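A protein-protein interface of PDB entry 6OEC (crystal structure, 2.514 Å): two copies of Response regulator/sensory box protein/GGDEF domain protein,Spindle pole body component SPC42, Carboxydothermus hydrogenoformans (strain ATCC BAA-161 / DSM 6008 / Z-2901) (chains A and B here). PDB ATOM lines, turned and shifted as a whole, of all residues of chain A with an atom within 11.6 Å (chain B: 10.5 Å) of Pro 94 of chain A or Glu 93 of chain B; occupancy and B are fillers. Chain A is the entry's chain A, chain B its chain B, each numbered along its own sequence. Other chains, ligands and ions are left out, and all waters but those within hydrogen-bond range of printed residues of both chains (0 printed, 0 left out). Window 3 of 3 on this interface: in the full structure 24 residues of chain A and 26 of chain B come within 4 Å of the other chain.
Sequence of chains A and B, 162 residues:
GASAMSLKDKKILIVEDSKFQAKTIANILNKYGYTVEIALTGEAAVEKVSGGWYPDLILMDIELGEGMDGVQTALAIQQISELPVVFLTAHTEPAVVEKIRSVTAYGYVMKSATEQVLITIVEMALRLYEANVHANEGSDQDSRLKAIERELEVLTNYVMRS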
ATOM      1  N   ILE A  62      41.069 -11.569 -32.948  1.00  0.00           N
ATOM      2  CA  ILE A  62      40.631 -10.299 -32.385  1.00  0.00           C
ATOM      3  C   ILE A  62      41.841  -9.408 -32.085  1.00  0.00           C
ATOM      4  O   ILE A  62      41.801  -8.194 -32.323  1.00  0.00           O
ATOM      5  CB  ILE A  62      39.727 -10.549 -31.148  1.00  0.00           C
ATOM      6  CG1 ILE A  62      38.786  -9.387 -30.934  1.00  0.00           C
ATOM      7  CG2 ILE A  62      40.497 -10.805 -29.852  1.00  0.00           C
ATOM      8  CD1 ILE A  62      37.933  -9.146 -32.132  1.00  0.00           C
ATOM      9  N   VAL A  71      39.596  -5.953 -35.014  1.00  0.00           N
ATOM     10  CA  VAL A  71      38.375  -5.196 -35.257  1.00  0.00           C
ATOM     11  C   VAL A  71      38.612  -4.071 -36.269  1.00  0.00           C
ATOM     12  O   VAL A  71      37.844  -3.906 -37.224  1.00  0.00           O
ATOM     13  CB  VAL A  71      37.835  -4.670 -33.923  1.00  0.00           C
ATOM     14  CG1 VAL A  71      36.727  -3.645 -34.164  1.00  0.00           C
ATOM     15  CG2 VAL A  71      37.370  -5.846 -33.103  1.00  0.00           C
ATOM     16  N   THR A  89      39.354 -15.835 -30.879  1.00  0.00           N
ATOM     17  CA  THR A  89      39.373 -15.126 -29.611  1.00  0.00           C
ATOM     18  C   THR A  89      39.721 -16.113 -28.505  1.00  0.00           C
ATOM     19  O   THR A  89      39.413 -17.312 -28.589  1.00  0.00           O
ATOM     20  CB  THR A  89      38.020 -14.436 -29.368  1.00  0.00           C
ATOM     21  OG1 THR A  89      38.098 -13.574 -28.241  1.00  0.00           O
ATOM     22  CG2 THR A  89      36.920 -15.455 -29.144  1.00  0.00           C
ATOM     23  N   ALA A  90      40.416 -15.624 -27.488  1.00  0.00           N
ATOM     24  CA  ALA A  90      40.653 -16.541 -26.385  1.00  0.00           C
ATOM     25  C   ALA A  90      39.476 -16.538 -25.437  1.00  0.00           C
ATOM     26  O   ALA A  90      39.118 -17.590 -24.902  1.00  0.00           O
ATOM     27  CB  ALA A  90      41.935 -16.206 -25.634  1.00  0.00           C
ATOM     28  N   HIS A  91      38.836 -15.385 -25.238  1.00  0.00           N
ATOM     29  CA  HIS A  91      37.892 -15.233 -24.133  1.00  0.00           C
ATOM     30  C   HIS A  91      36.697 -14.376 -24.518  1.00  0.00           C
ATOM     31  O   HIS A  91      36.857 -13.194 -24.860  1.00  0.00           O
ATOM     32  CB  HIS A  91      38.614 -14.644 -22.922  1.00  0.00           C
ATOM     33  CG  HIS A  91      39.669 -15.556 -22.378  1.00  0.00           C
ATOM     34  ND1 HIS A  91      39.608 -16.926 -22.532  1.00  0.00           N
ATOM     35  CD2 HIS A  91      40.808 -15.303 -21.695  1.00  0.00           C
ATOM     36  CE1 HIS A  91      40.670 -17.478 -21.976  1.00  0.00           C
ATOM     37  NE2 HIS A  91      41.414 -16.515 -21.459  1.00  0.00           N
ATOM     38  N   THR A  92      35.505 -14.967 -24.383  1.00  0.00           N
ATOM     39  CA  THR A  92      34.237 -14.307 -24.663  1.00  0.00           C
ATOM     40  C   THR A  92      33.779 -13.341 -23.562  1.00  0.00           C
ATOM     41  O   THR A  92      32.603 -13.359 -23.171  1.00  0.00           O
ATOM     42  CB  THR A  92      33.156 -15.363 -24.877  1.00  0.00           C
ATOM     43  OG1 THR A  92      32.823 -15.956 -23.617  1.00  0.00           O
ATOM     44  CG2 THR A  92      33.665 -16.453 -25.770  1.00  0.00           C
ATOM     45  N   GLU A  93      34.663 -12.471 -23.073  1.00  0.00           N
ATOM     46  CA  GLU A  93      34.220 -11.425 -22.157  1.00  0.00           C
ATOM     47  C   GLU A  93      33.313 -10.418 -22.874  1.00  0.00           C
ATOM     48  O   GLU A  93      33.495 -10.146 -24.069  1.00  0.00           O
ATOM     49  CB  GLU A  93      35.418 -10.705 -21.552  1.00  0.00           C
ATOM     50  CG  GLU A  93      36.485 -11.657 -21.019  1.00  0.00           C
ATOM     51  CD  GLU A  93      35.987 -12.554 -19.853  1.00  0.00           C
ATOM     52  OE1 GLU A  93      35.167 -12.054 -19.017  1.00  0.00           O
ATOM     53  OE2 GLU A  93      36.428 -13.755 -19.785  1.00  0.00           O
ATOM     54  N   PRO A  94      32.333  -9.837 -22.162  1.00  0.00           N
ATOM     55  CA  PRO A  94      31.354  -8.946 -22.825  1.00  0.00           C
ATOM     56  C   PRO A  94      31.935  -7.874 -23.734  1.00  0.00           C
ATOM     57  O   PRO A  94      31.515  -7.776 -24.895  1.00  0.00           O
ATOM     58  CB  PRO A  94      30.602  -8.339 -21.637  1.00  0.00           C
ATOM     59  CG  PRO A  94      30.610  -9.435 -20.611  1.00  0.00           C
ATOM     60  CD  PRO A  94      31.940 -10.155 -20.775  1.00  0.00           C
ATOM     61  N   ALA A  95      32.888  -7.071 -23.260  1.00  0.00           N
ATOM     62  CA  ALA A  95      33.434  -6.009 -24.108  1.00  0.00           C
ATOM     63  C   ALA A  95      33.984  -6.570 -25.411  1.00  0.00           C
ATOM     64  O   ALA A  95      33.850  -5.946 -26.472  1.00  0.00           O
ATOM     65  CB  ALA A  95      34.529  -5.233 -23.377  1.00  0.00           C
ATOM     66  N   VAL A  96      34.612  -7.746 -25.348  1.00  0.00           N
ATOM     67  CA  VAL A  96      35.189  -8.346 -26.546  1.00  0.00           C
ATOM     68  C   VAL A  96      34.090  -8.830 -27.485  1.00  0.00           C
ATOM     69  O   VAL A  96      34.125  -8.569 -28.697  1.00  0.00           O
ATOM     70  CB  VAL A  96      36.152  -9.481 -26.165  1.00  0.00           C
ATOM     71  CG1 VAL A  96      36.594 -10.242 -27.397  1.00  0.00           C
ATOM     72  CG2 VAL A  96      37.355  -8.891 -25.495  1.00  0.00           C
ATOM     73  N   VAL A  97      33.096  -9.541 -26.936  1.00  0.00           N
ATOM     74  CA  VAL A  97      32.021 -10.075 -27.762  1.00  0.00           C
ATOM     75  C   VAL A  97      31.213  -8.953 -28.408  1.00  0.00           C
ATOM     76  O   VAL A  97      30.718  -9.102 -29.525  1.00  0.00           O
ATOM     77  CB  VAL A  97      31.158 -11.014 -26.904  1.00  0.00           C
ATOM     78  CG1 VAL A  97      29.926 -11.448 -27.636  1.00  0.00           C
ATOM     79  CG2 VAL A  97      31.957 -12.206 -26.545  1.00  0.00           C
ATOM     80  N   GLU A  98      31.104  -7.800 -27.746  1.00  0.00           N
ATOM     81  CA  GLU A  98      30.413  -6.664 -28.357  1.00  0.00           C
ATOM     82  C   GLU A  98      31.194  -6.093 -29.535  1.00  0.00           C
ATOM     83  O   GLU A  98      30.597  -5.750 -30.560  1.00  0.00           O
ATOM     84  CB  GLU A  98      30.159  -5.573 -27.322  1.00  0.00           C
ATOM     85  CG  GLU A  98      29.135  -5.949 -26.297  1.00  0.00           C
ATOM     86  CD  GLU A  98      29.138  -5.023 -25.077  1.00  0.00           C
ATOM     87  OE1 GLU A  98      29.592  -3.843 -25.208  1.00  0.00           O
ATOM     88  OE2 GLU A  98      28.673  -5.498 -23.999  1.00  0.00           O
ATOM     89  N   LYS A  99      32.519  -5.934 -29.398  1.00  0.00           N
ATOM     90  CA  LYS A  99      33.329  -5.513 -30.540  1.00  0.00           C
ATOM     91  C   LYS A  99      33.155  -6.479 -31.695  1.00  0.00           C
ATOM     92  O   LYS A  99      32.941  -6.060 -32.836  1.00  0.00           O
ATOM     93  CB  LYS A  99      34.806  -5.411 -30.172  1.00  0.00           C
ATOM     94  CG  LYS A  99      35.191  -4.270 -29.254  1.00  0.00           C
ATOM     95  CD  LYS A  99      36.545  -4.643 -28.666  1.00  0.00           C
ATOM     96  CE  LYS A  99      37.476  -3.461 -28.386  1.00  0.00           C
ATOM     97  NZ  LYS A  99      38.770  -4.019 -27.876  1.00  0.00           N
ATOM     98  N   ILE A 100      33.230  -7.779 -31.410  1.00  0.00           N
ATOM     99  CA  ILE A 100      33.100  -8.768 -32.473  1.00  0.00           C
ATOM    100  C   ILE A 100      31.741  -8.641 -33.142  1.00  0.00           C
ATOM    101  O   ILE A 100      31.633  -8.609 -34.375  1.00  0.00           O
ATOM    102  CB  ILE A 100      33.309 -10.186 -31.929  1.00  0.00           C
ATOM    103  CG1 ILE A 100      34.757 -10.408 -31.513  1.00  0.00           C
ATOM    104  CG2 ILE A 100      32.924 -11.193 -32.978  1.00  0.00           C
ATOM    105  CD1 ILE A 100      34.922 -11.638 -30.570  1.00  0.00           C
ATOM    106  N   ARG A 101      30.678  -8.561 -32.339  1.00  0.00           N
ATOM    107  CA  ARG A 101      29.334  -8.567 -32.909  1.00  0.00           C
ATOM    108  C   ARG A 101      29.034  -7.290 -33.666  1.00  0.00           C
ATOM    109  O   ARG A 101      28.087  -7.257 -34.465  1.00  0.00           O
ATOM    110  CB  ARG A 101      28.297  -8.794 -31.808  1.00  0.00           C
ATOM    111  CG  ARG A 101      28.210 -10.232 -31.460  1.00  0.00           C
ATOM    112  CD  ARG A 101      27.151 -10.535 -30.435  1.00  0.00           C
ATOM    113  NE  ARG A 101      27.556 -11.708 -29.680  1.00  0.00           N
ATOM    114  CZ  ARG A 101      27.164 -12.944 -29.947  1.00  0.00           C
ATOM    115  NH1 ARG A 101      26.306 -13.153 -30.944  1.00  0.00           N
ATOM    116  NH2 ARG A 101      27.626 -13.958 -29.197  1.00  0.00           N
ATOM    117  N   SER A 102      29.835  -6.250 -33.452  1.00  0.00           N
ATOM    118  CA  SER A 102      29.584  -4.985 -34.115  1.00  0.00           C
ATOM    119  C   SER A 102      30.156  -4.929 -35.526  1.00  0.00           C
ATOM    120  O   SER A 102      29.627  -4.193 -36.369  1.00  0.00           O
ATOM    121  CB  SER A 102      30.144  -3.858 -33.270  1.00  0.00           C
ATOM    122  OG  SER A 102      29.191  -3.526 -32.296  1.00  0.00           O
ATOM    123  N   VAL A 103      31.206  -5.701 -35.813  1.00  0.00           N
ATOM    124  CA  VAL A 103      31.868  -5.639 -37.112  1.00  0.00           C
ATOM    125  C   VAL A 103      31.636  -6.870 -37.972  1.00  0.00           C
ATOM    126  O   VAL A 103      31.933  -6.815 -39.171  1.00  0.00           O
ATOM    127  CB  VAL A 103      33.386  -5.382 -36.973  1.00  0.00           C
ATOM    128  CG1 VAL A 103      33.610  -4.067 -36.254  1.00  0.00           C
ATOM    129  CG2 VAL A 103      34.102  -6.557 -36.239  1.00  0.00           C
ATOM    130  N   TYR A 108      32.377 -16.067 -34.241  1.00  0.00           N
ATOM    131  CA  TYR A 108      33.756 -16.277 -33.822  1.00  0.00           C
ATOM    132  C   TYR A 108      34.005 -17.743 -33.481  1.00  0.00           C
ATOM    133  O   TYR A 108      33.087 -18.567 -33.493  1.00  0.00           O
ATOM    134  CB  TYR A 108      34.092 -15.369 -32.643  1.00  0.00           C
ATOM    135  CG  TYR A 108      33.288 -15.634 -31.410  1.00  0.00           C
ATOM    136  CD1 TYR A 108      33.740 -16.533 -30.451  1.00  0.00           C
ATOM    137  CD2 TYR A 108      32.094 -14.980 -31.179  1.00  0.00           C
ATOM    138  CE1 TYR A 108      33.028 -16.779 -29.309  1.00  0.00           C
ATOM    139  CE2 TYR A 108      31.369 -15.226 -30.027  1.00  0.00           C
ATOM    140  CZ  TYR A 108      31.844 -16.132 -29.101  1.00  0.00           C
ATOM    141  OH  TYR A 108      31.154 -16.393 -27.942  1.00  0.00           O
ATOM    142  N   MET A 110      36.536 -20.022 -30.545  1.00  0.00           N
ATOM    143  CA  MET A 110      37.461 -20.030 -29.417  1.00  0.00           C
ATOM    144  C   MET A 110      38.796 -20.588 -29.871  1.00  0.00           C
ATOM    145  O   MET A 110      38.843 -21.629 -30.527  1.00  0.00           O
ATOM    146  CB  MET A 110      36.919 -20.902 -28.288  1.00  0.00           C
ATOM    147  CG  MET A 110      35.541 -20.564 -27.821  1.00  0.00           C
ATOM    148  SD  MET A 110      35.401 -18.801 -27.472  1.00  0.00           S
ATOM    149  CE  MET A 110      36.615 -18.580 -26.184  1.00  0.00           C
ATOM    150  N   ILE B  62      15.456  -4.161 -26.355  1.00  0.00           N
ATOM    151  CA  ILE B  62      15.099  -4.833 -25.094  1.00  0.00           C
ATOM    152  C   ILE B  62      14.599  -3.870 -24.028  1.00  0.00           C
ATOM    153  O   ILE B  62      14.021  -4.314 -23.031  1.00  0.00           O
ATOM    154  CB  ILE B  62      16.208  -5.645 -24.385  1.00  0.00           C
ATOM    155  CG1 ILE B  62      17.612  -5.149 -24.687  1.00  0.00           C
ATOM    156  CG2 ILE B  62      16.006  -7.112 -24.549  1.00  0.00           C
ATOM    157  CD1 ILE B  62      17.995  -3.947 -23.790  1.00  0.00           C
ATOM    158  N   GLU B  63      14.837  -2.576 -24.173  1.00  0.00           N
ATOM    159  CA  GLU B  63      14.419  -1.595 -23.182  1.00  0.00           C
ATOM    160  C   GLU B  63      13.578  -0.558 -23.895  1.00  0.00           C
ATOM    161  O   GLU B  63      14.042   0.059 -24.857  1.00  0.00           O
ATOM    162  CB  GLU B  63      15.624  -0.960 -22.491  1.00  0.00           C
ATOM    163  CG  GLU B  63      16.087  -1.727 -21.261  1.00  0.00           C
ATOM    164  CD  GLU B  63      17.543  -1.447 -20.897  1.00  0.00           C
ATOM    165  OE1 GLU B  63      18.234  -2.384 -20.407  1.00  0.00           O
ATOM    166  OE2 GLU B  63      17.994  -0.290 -21.109  1.00  0.00           O
ATOM    167  N   THR B  89      20.317  -4.415 -28.738  1.00  0.00           N
ATOM    168  CA  THR B  89      20.811  -4.220 -27.383  1.00  0.00           C
ATOM    169  C   THR B  89      22.082  -3.365 -27.375  1.00  0.00           C
ATOM    170  O   THR B  89      22.944  -3.480 -28.270  1.00  0.00           O
ATOM    171  CB  THR B  89      21.057  -5.561 -26.711  1.00  0.00           C
ATOM    172  OG1 THR B  89      21.488  -5.344 -25.365  1.00  0.00           O
ATOM    173  CG2 THR B  89      22.125  -6.324 -27.460  1.00  0.00           C
ATOM    174  N   ALA B  90      22.173  -2.486 -26.359  1.00  0.00           N
ATOM    175  CA  ALA B  90      23.389  -1.706 -26.140  1.00  0.00           C
ATOM    176  C   ALA B  90      24.570  -2.605 -25.813  1.00  0.00           C
ATOM    177  O   ALA B  90      25.657  -2.439 -26.378  1.00  0.00           O
ATOM    178  CB  ALA B  90      23.179  -0.690 -25.019  1.00  0.00           C
ATOM    179  N   HIS B  91      24.383  -3.574 -24.908  1.00  0.00           N
ATOM    180  CA  HIS B  91      25.483  -4.450 -24.493  1.00  0.00           C
ATOM    181  C   HIS B  91      25.007  -5.883 -24.286  1.00  0.00           C
ATOM    182  O   HIS B  91      23.823  -6.213 -24.440  1.00  0.00           O
ATOM    183  CB  HIS B  91      26.153  -3.977 -23.198  1.00  0.00           C
ATOM    184  CG  HIS B  91      26.549  -2.540 -23.217  1.00  0.00           C
ATOM    185  ND1 HIS B  91      27.628  -2.075 -23.938  1.00  0.00           N
ATOM    186  CD2 HIS B  91      26.006  -1.461 -22.606  1.00  0.00           C
ATOM    187  CE1 HIS B  91      27.730  -0.769 -23.766  1.00  0.00           C
ATOM    188  NE2 HIS B  91      26.762  -0.373 -22.957  1.00  0.00           N
ATOM    189  N   THR B  92      25.955  -6.699 -23.832  1.00  0.00           N
ATOM    190  CA  THR B  92      25.934  -8.152 -23.872  1.00  0.00           C
ATOM    191  C   THR B  92      26.162  -8.705 -22.468  1.00  0.00           C
ATOM    192  O   THR B  92      26.820  -9.723 -22.257  1.00  0.00           O
ATOM    193  CB  THR B  92      26.970  -8.613 -24.900  1.00  0.00           C
ATOM    194  OG1 THR B  92      26.514  -8.183 -26.186  1.00  0.00           O
ATOM    195  CG2 THR B  92      27.167 -10.090 -24.972  1.00  0.00           C
ATOM    196  N   GLU B  93      25.626  -8.025 -21.469  1.00  0.00           N
ATOM    197  CA  GLU B  93      25.758  -8.556 -20.122  1.00  0.00           C
ATOM    198  C   GLU B  93      24.966  -9.858 -19.999  1.00  0.00           C
ATOM    199  O   GLU B  93      23.874  -9.991 -20.577  1.00  0.00           O
ATOM    200  CB  GLU B  93      25.296  -7.541 -19.076  1.00  0.00           C
ATOM    201  CG  GLU B  93      26.253  -6.344 -18.893  1.00  0.00           C
ATOM    202  CD  GLU B  93      27.754  -6.731 -18.946  1.00  0.00           C
ATOM    203  OE1 GLU B  93      28.189  -7.725 -18.309  1.00  0.00           O
ATOM    204  OE2 GLU B  93      28.508  -6.016 -19.646  1.00  0.00           O
ATOM    205  N   PRO B  94      25.501 -10.843 -19.281  1.00  0.00           N
ATOM    206  CA  PRO B  94      24.836 -12.154 -19.226  1.00  0.00           C
ATOM    207  C   PRO B  94      23.379 -12.065 -18.829  1.00  0.00           C
ATOM    208  O   PRO B  94      22.556 -12.844 -19.329  1.00  0.00           O
ATOM    209  CB  PRO B  94      25.664 -12.922 -18.184  1.00  0.00           C
ATOM    210  CG  PRO B  94      26.984 -12.236 -18.191  1.00  0.00           C
ATOM    211  CD  PRO B  94      26.726 -10.797 -18.466  1.00  0.00           C
ATOM    212  N   ALA B  95      23.023 -11.129 -17.956  1.00  0.00           N
ATOM    213  CA  ALA B  95      21.636 -11.049 -17.538  1.00  0.00           C
ATOM    214  C   ALA B  95      20.742 -10.692 -18.716  1.00  0.00           C
ATOM    215  O   ALA B  95      19.678 -11.297 -18.890  1.00  0.00           O
ATOM    216  CB  ALA B  95      21.486 -10.043 -16.399  1.00  0.00           C
ATOM    217  N   VAL B  96      21.170  -9.741 -19.556  1.00  0.00           N
ATOM    218  CA  VAL B  96      20.378  -9.380 -20.735  1.00  0.00           C
ATOM    219  C   VAL B  96      20.366 -10.526 -21.738  1.00  0.00           C
ATOM    220  O   VAL B  96      19.297 -10.985 -22.149  1.00  0.00           O
ATOM    221  CB  VAL B  96      20.896  -8.077 -21.378  1.00  0.00           C
ATOM    222  CG1 VAL B  96      20.150  -7.793 -22.699  1.00  0.00           C
ATOM    223  CG2 VAL B  96      20.733  -6.903 -20.431  1.00  0.00           C
ATOM    224  N   VAL B  97      21.549 -11.015 -22.139  1.00  0.00           N
ATOM    225  CA  VAL B  97      21.608 -12.127 -23.097  1.00  0.00           C
ATOM    226  C   VAL B  97      20.757 -13.317 -22.645  1.00  0.00           C
ATOM    227  O   VAL B  97      20.158 -14.012 -23.478  1.00  0.00           O
ATOM    228  CB  VAL B  97      23.077 -12.550 -23.354  1.00  0.00           C
ATOM    229  CG1 VAL B  97      23.129 -13.839 -24.176  1.00  0.00           C
ATOM    230  CG2 VAL B  97      23.831 -11.440 -24.069  1.00  0.00           C
ATOM    231  N   GLU B  98      20.683 -13.570 -21.332  1.00  0.00           N
ATOM    232  CA  GLU B  98      19.841 -14.652 -20.823  1.00  0.00           C
ATOM    233  C   GLU B  98      18.384 -14.479 -21.217  1.00  0.00           C
ATOM    234  O   GLU B  98      17.733 -15.439 -21.633  1.00  0.00           O
ATOM    235  CB  GLU B  98      19.945 -14.727 -19.314  1.00  0.00           C
ATOM    236  CG  GLU B  98      20.873 -15.791 -18.893  1.00  0.00           C
ATOM    237  CD  GLU B  98      21.474 -15.512 -17.544  1.00  0.00           C
ATOM    238  OE1 GLU B  98      20.673 -15.199 -16.613  1.00  0.00           O
ATOM    239  OE2 GLU B  98      22.736 -15.600 -17.457  1.00  0.00           O
ATOM    240  N   LYS B  99      17.847 -13.266 -21.067  1.00  0.00           N
ATOM    241  CA  LYS B  99      16.437 -13.037 -21.360  1.00  0.00           C
ATOM    242  C   LYS B  99      16.177 -13.120 -22.855  1.00  0.00           C
ATOM    243  O   LYS B  99      15.242 -13.809 -23.278  1.00  0.00           O
ATOM    244  CB  LYS B  99      15.979 -11.687 -20.802  1.00  0.00           C
ATOM    245  CG  LYS B  99      16.474 -11.357 -19.381  1.00  0.00           C
ATOM    246  CD  LYS B  99      16.124 -12.453 -18.322  1.00  0.00           C
ATOM    247  CE  LYS B  99      16.591 -12.113 -16.869  1.00  0.00           C
ATOM    248  NZ  LYS B  99      18.057 -12.384 -16.549  1.00  0.00           N
ATOM    249  N   ILE B 100      17.024 -12.455 -23.668  1.00  0.00           N
ATOM    250  CA  ILE B 100      16.910 -12.478 -25.134  1.00  0.00           C
ATOM    251  C   ILE B 100      16.832 -13.911 -25.649  1.00  0.00           C
ATOM    252  O   ILE B 100      15.944 -14.257 -26.444  1.00  0.00           O
ATOM    253  CB  ILE B 100      18.100 -11.740 -25.789  1.00  0.00           C
ATOM    254  CG1 ILE B 100      18.050 -10.221 -25.578  1.00  0.00           C
ATOM    255  CG2 ILE B 100      18.192 -12.058 -27.283  1.00  0.00           C
ATOM    256  CD1 ILE B 100      19.294  -9.509 -26.069  1.00  0.00           C
ATOM    257  N   ARG B 101      17.781 -14.764 -25.225  1.00  0.00           N
ATOM    258  CA  ARG B 101      17.858 -16.118 -25.766  1.00  0.00           C
ATOM    259  C   ARG B 101      16.712 -16.999 -25.304  1.00  0.00           C
ATOM    260  O   ARG B 101      16.497 -18.062 -25.890  1.00  0.00           O
ATOM    261  CB  ARG B 101      19.178 -16.781 -25.394  1.00  0.00           C
ATOM    262  CG  ARG B 101      20.407 -16.022 -25.840  1.00  0.00           C
ATOM    263  CD  ARG B 101      21.301 -16.891 -26.694  1.00  0.00           C
ATOM    264  NE  ARG B 101      22.570 -16.252 -27.029  1.00  0.00           N
ATOM    265  CZ  ARG B 101      22.798 -15.549 -28.140  1.00  0.00           C
ATOM    266  NH1 ARG B 101      21.841 -15.364 -29.054  1.00  0.00           N
ATOM    267  NH2 ARG B 101      23.999 -15.013 -28.333  1.00  0.00           N
ATOM    268  N   TYR B 108      20.392 -11.353 -31.719  1.00  0.00           N
ATOM    269  CA  TYR B 108      20.349  -9.917 -31.475  1.00  0.00           C
ATOM    270  C   TYR B 108      21.364  -9.204 -32.349  1.00  0.00           C
ATOM    271  O   TYR B 108      22.181  -9.827 -33.028  1.00  0.00           O
ATOM    272  CB  TYR B 108      20.590  -9.600 -30.002  1.00  0.00           C
ATOM    273  CG  TYR B 108      21.899 -10.095 -29.433  1.00  0.00           C
ATOM    274  CD1 TYR B 108      22.008 -11.367 -28.908  1.00  0.00           C
ATOM    275  CD2 TYR B 108      23.007  -9.261 -29.365  1.00  0.00           C
ATOM    276  CE1 TYR B 108      23.187 -11.816 -28.350  1.00  0.00           C
ATOM    277  CE2 TYR B 108      24.198  -9.700 -28.819  1.00  0.00           C
ATOM    278  CZ  TYR B 108      24.284 -10.981 -28.307  1.00  0.00           C
ATOM    279  OH  TYR B 108      25.472 -11.432 -27.757  1.00  0.00           O
ATOM    280  N   MET B 110      23.901  -5.524 -32.076  1.00  0.00           N
ATOM    281  CA  MET B 110      24.355  -4.440 -31.215  1.00  0.00           C
ATOM    282  C   MET B 110      23.802  -3.114 -31.719  1.00  0.00           C
ATOM    283  O   MET B 110      23.664  -2.899 -32.927  1.00  0.00           O
ATOM    284  CB  MET B 110      25.877  -4.392 -31.176  1.00  0.00           C
ATOM    285  CG  MET B 110      26.531  -5.709 -30.792  1.00  0.00           C
ATOM    286  SD  MET B 110      25.874  -6.440 -29.288  1.00  0.00           S
ATOM    287  CE  MET B 110      26.147  -5.088 -28.136  1.00  0.00           C
ATOM    288  N   SER B 112      25.447  -0.606 -31.675  1.00  0.00           N
ATOM    289  CA  SER B 112      26.633  -0.022 -32.290  1.00  0.00           C
ATOM    290  C   SER B 112      27.119  -0.775 -33.533  1.00  0.00           C
ATOM    291  O   SER B 112      28.139  -0.387 -34.108  1.00  0.00           O
ATOM    292  CB  SER B 112      27.775   0.037 -31.271  1.00  0.00           C
ATOM    293  OG  SER B 112      28.271  -1.263 -31.006  1.00  0.00           O
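Glu 93 of chain B touches one residue of chain A. No residue of chain B comes within 4 Å of Glu 93 of chain A. No residue of chain B comes within 4 Å of Val 97 of chain A. Of the printed residues of chain B, Glu 98 of chain A touches His 91, Thr 92 and Met 110. His 91 of chain B touches just one residue of chain A: Glu 98. Of chain A, only Glu 98 (3.0 Å) comes within 4 Å of Thr 92 of chain B. No residue of chain A comes within 4 Å of Pro 94 of chain B. No residue of chain A comes within 4 Å of Ala 95 of chain B. No residue of chain A comes within 4 Å of Val 97 of chain B. Printed residues of chain A within 4 Å of Tyr 108 of chain B: Arg 101 (2.8 Å). Of the printed residues of chain A, Ser 112 of chain B touches Ser 102 (2.8 Å). Of the printed residues of chain B, Arg 101 of chain A touches Arg 101, Tyr 108 and Met 110. Thr 89 of chain B touches none of the printed residues of chain A. Lys 99 of chain B touches none of the printed residues of chain A.
O of Glu 98 of chain A is in hydrogen-bond range of OG of Ser 102 of chain A. The side-chain hydroxyl (OG1) of Thr 89 of chain B lies within hydrogen-bond range of the backbone carbonyl oxygen (O) of His 91 of chain B, 2.7 Å away. The side-chain hydroxyl (OG1) of Thr 92 of chain B is in hydrogen-bond range of the side-chain sulfur (SD) of Met 110 of chain B (3.6 Å).
Among the printed residues, merely in contact across the chains: Ser 102 of chain A with Met 110 of chain B (3.6 Å), Glu 98 of chain A with Met 110 of chain B (3.6 Å), Arg 101 of chain A with Met 110 of chain B (3.7 Å), Pro 94 of chain A with Glu 93 of chain B (3.7 Å) and Arg 101 of chain A with Arg 101 of chain B (3.9 Å).
Of the 19 printed residues of chain A, 4 touch a printed residue of chain B. Printed residues of chain A that touch a printed residue of chain B: Pro 94, Glu 98, Arg 101 and Ser 102. Printed residues of chain B that touch a printed residue of chain A: His 91, Thr 92, Glu 93, Arg 101, Tyr 108, Met 110 and Ser 112. Hydrophobic or aromatic side chains of chain B within 4 Å of the printed part of chain A: His 91, Tyr 108 and Met 110.
Pro 94 of chain A touches Glu 93 of chain B, but with the chains exchanged Glu 93 of chain A does not touch Pro 94 of chain B (7.9 Å). Glu 98 of chain A touches His 91 of chain B, but with the chains exchanged His 91 of chain A does not touch Glu 98 of chain B (15.7 Å). Glu 98 of chain A touches Thr 92 of chain B, but with the chains exchanged Thr 92 of chain A does not touch Glu 98 of chain B (11.6 Å). Arg 101 of chain A touches its own counterpart, Arg 101 of chain B. Of the 9 pairs that touch across the chains among the printed residues, 1 has its exchanged pair printed and touching as well.
ND1 of His 91 of chain B lies within hydrogen-bond range of OE1 of Glu 98 of chain A (2.9 Å). OE2 of Glu 98 of chain A sits at hydrogen-bond distance from N of Thr 92 of chain B (3.0 Å). NE of Arg 101 of chain A lies within hydrogen-bond range of OH of Tyr 108 of chain B, at 2.8 Å. OG of Ser 112 of chain B lies within hydrogen-bond range of OG of Ser 102 of chain A (2.8 Å).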
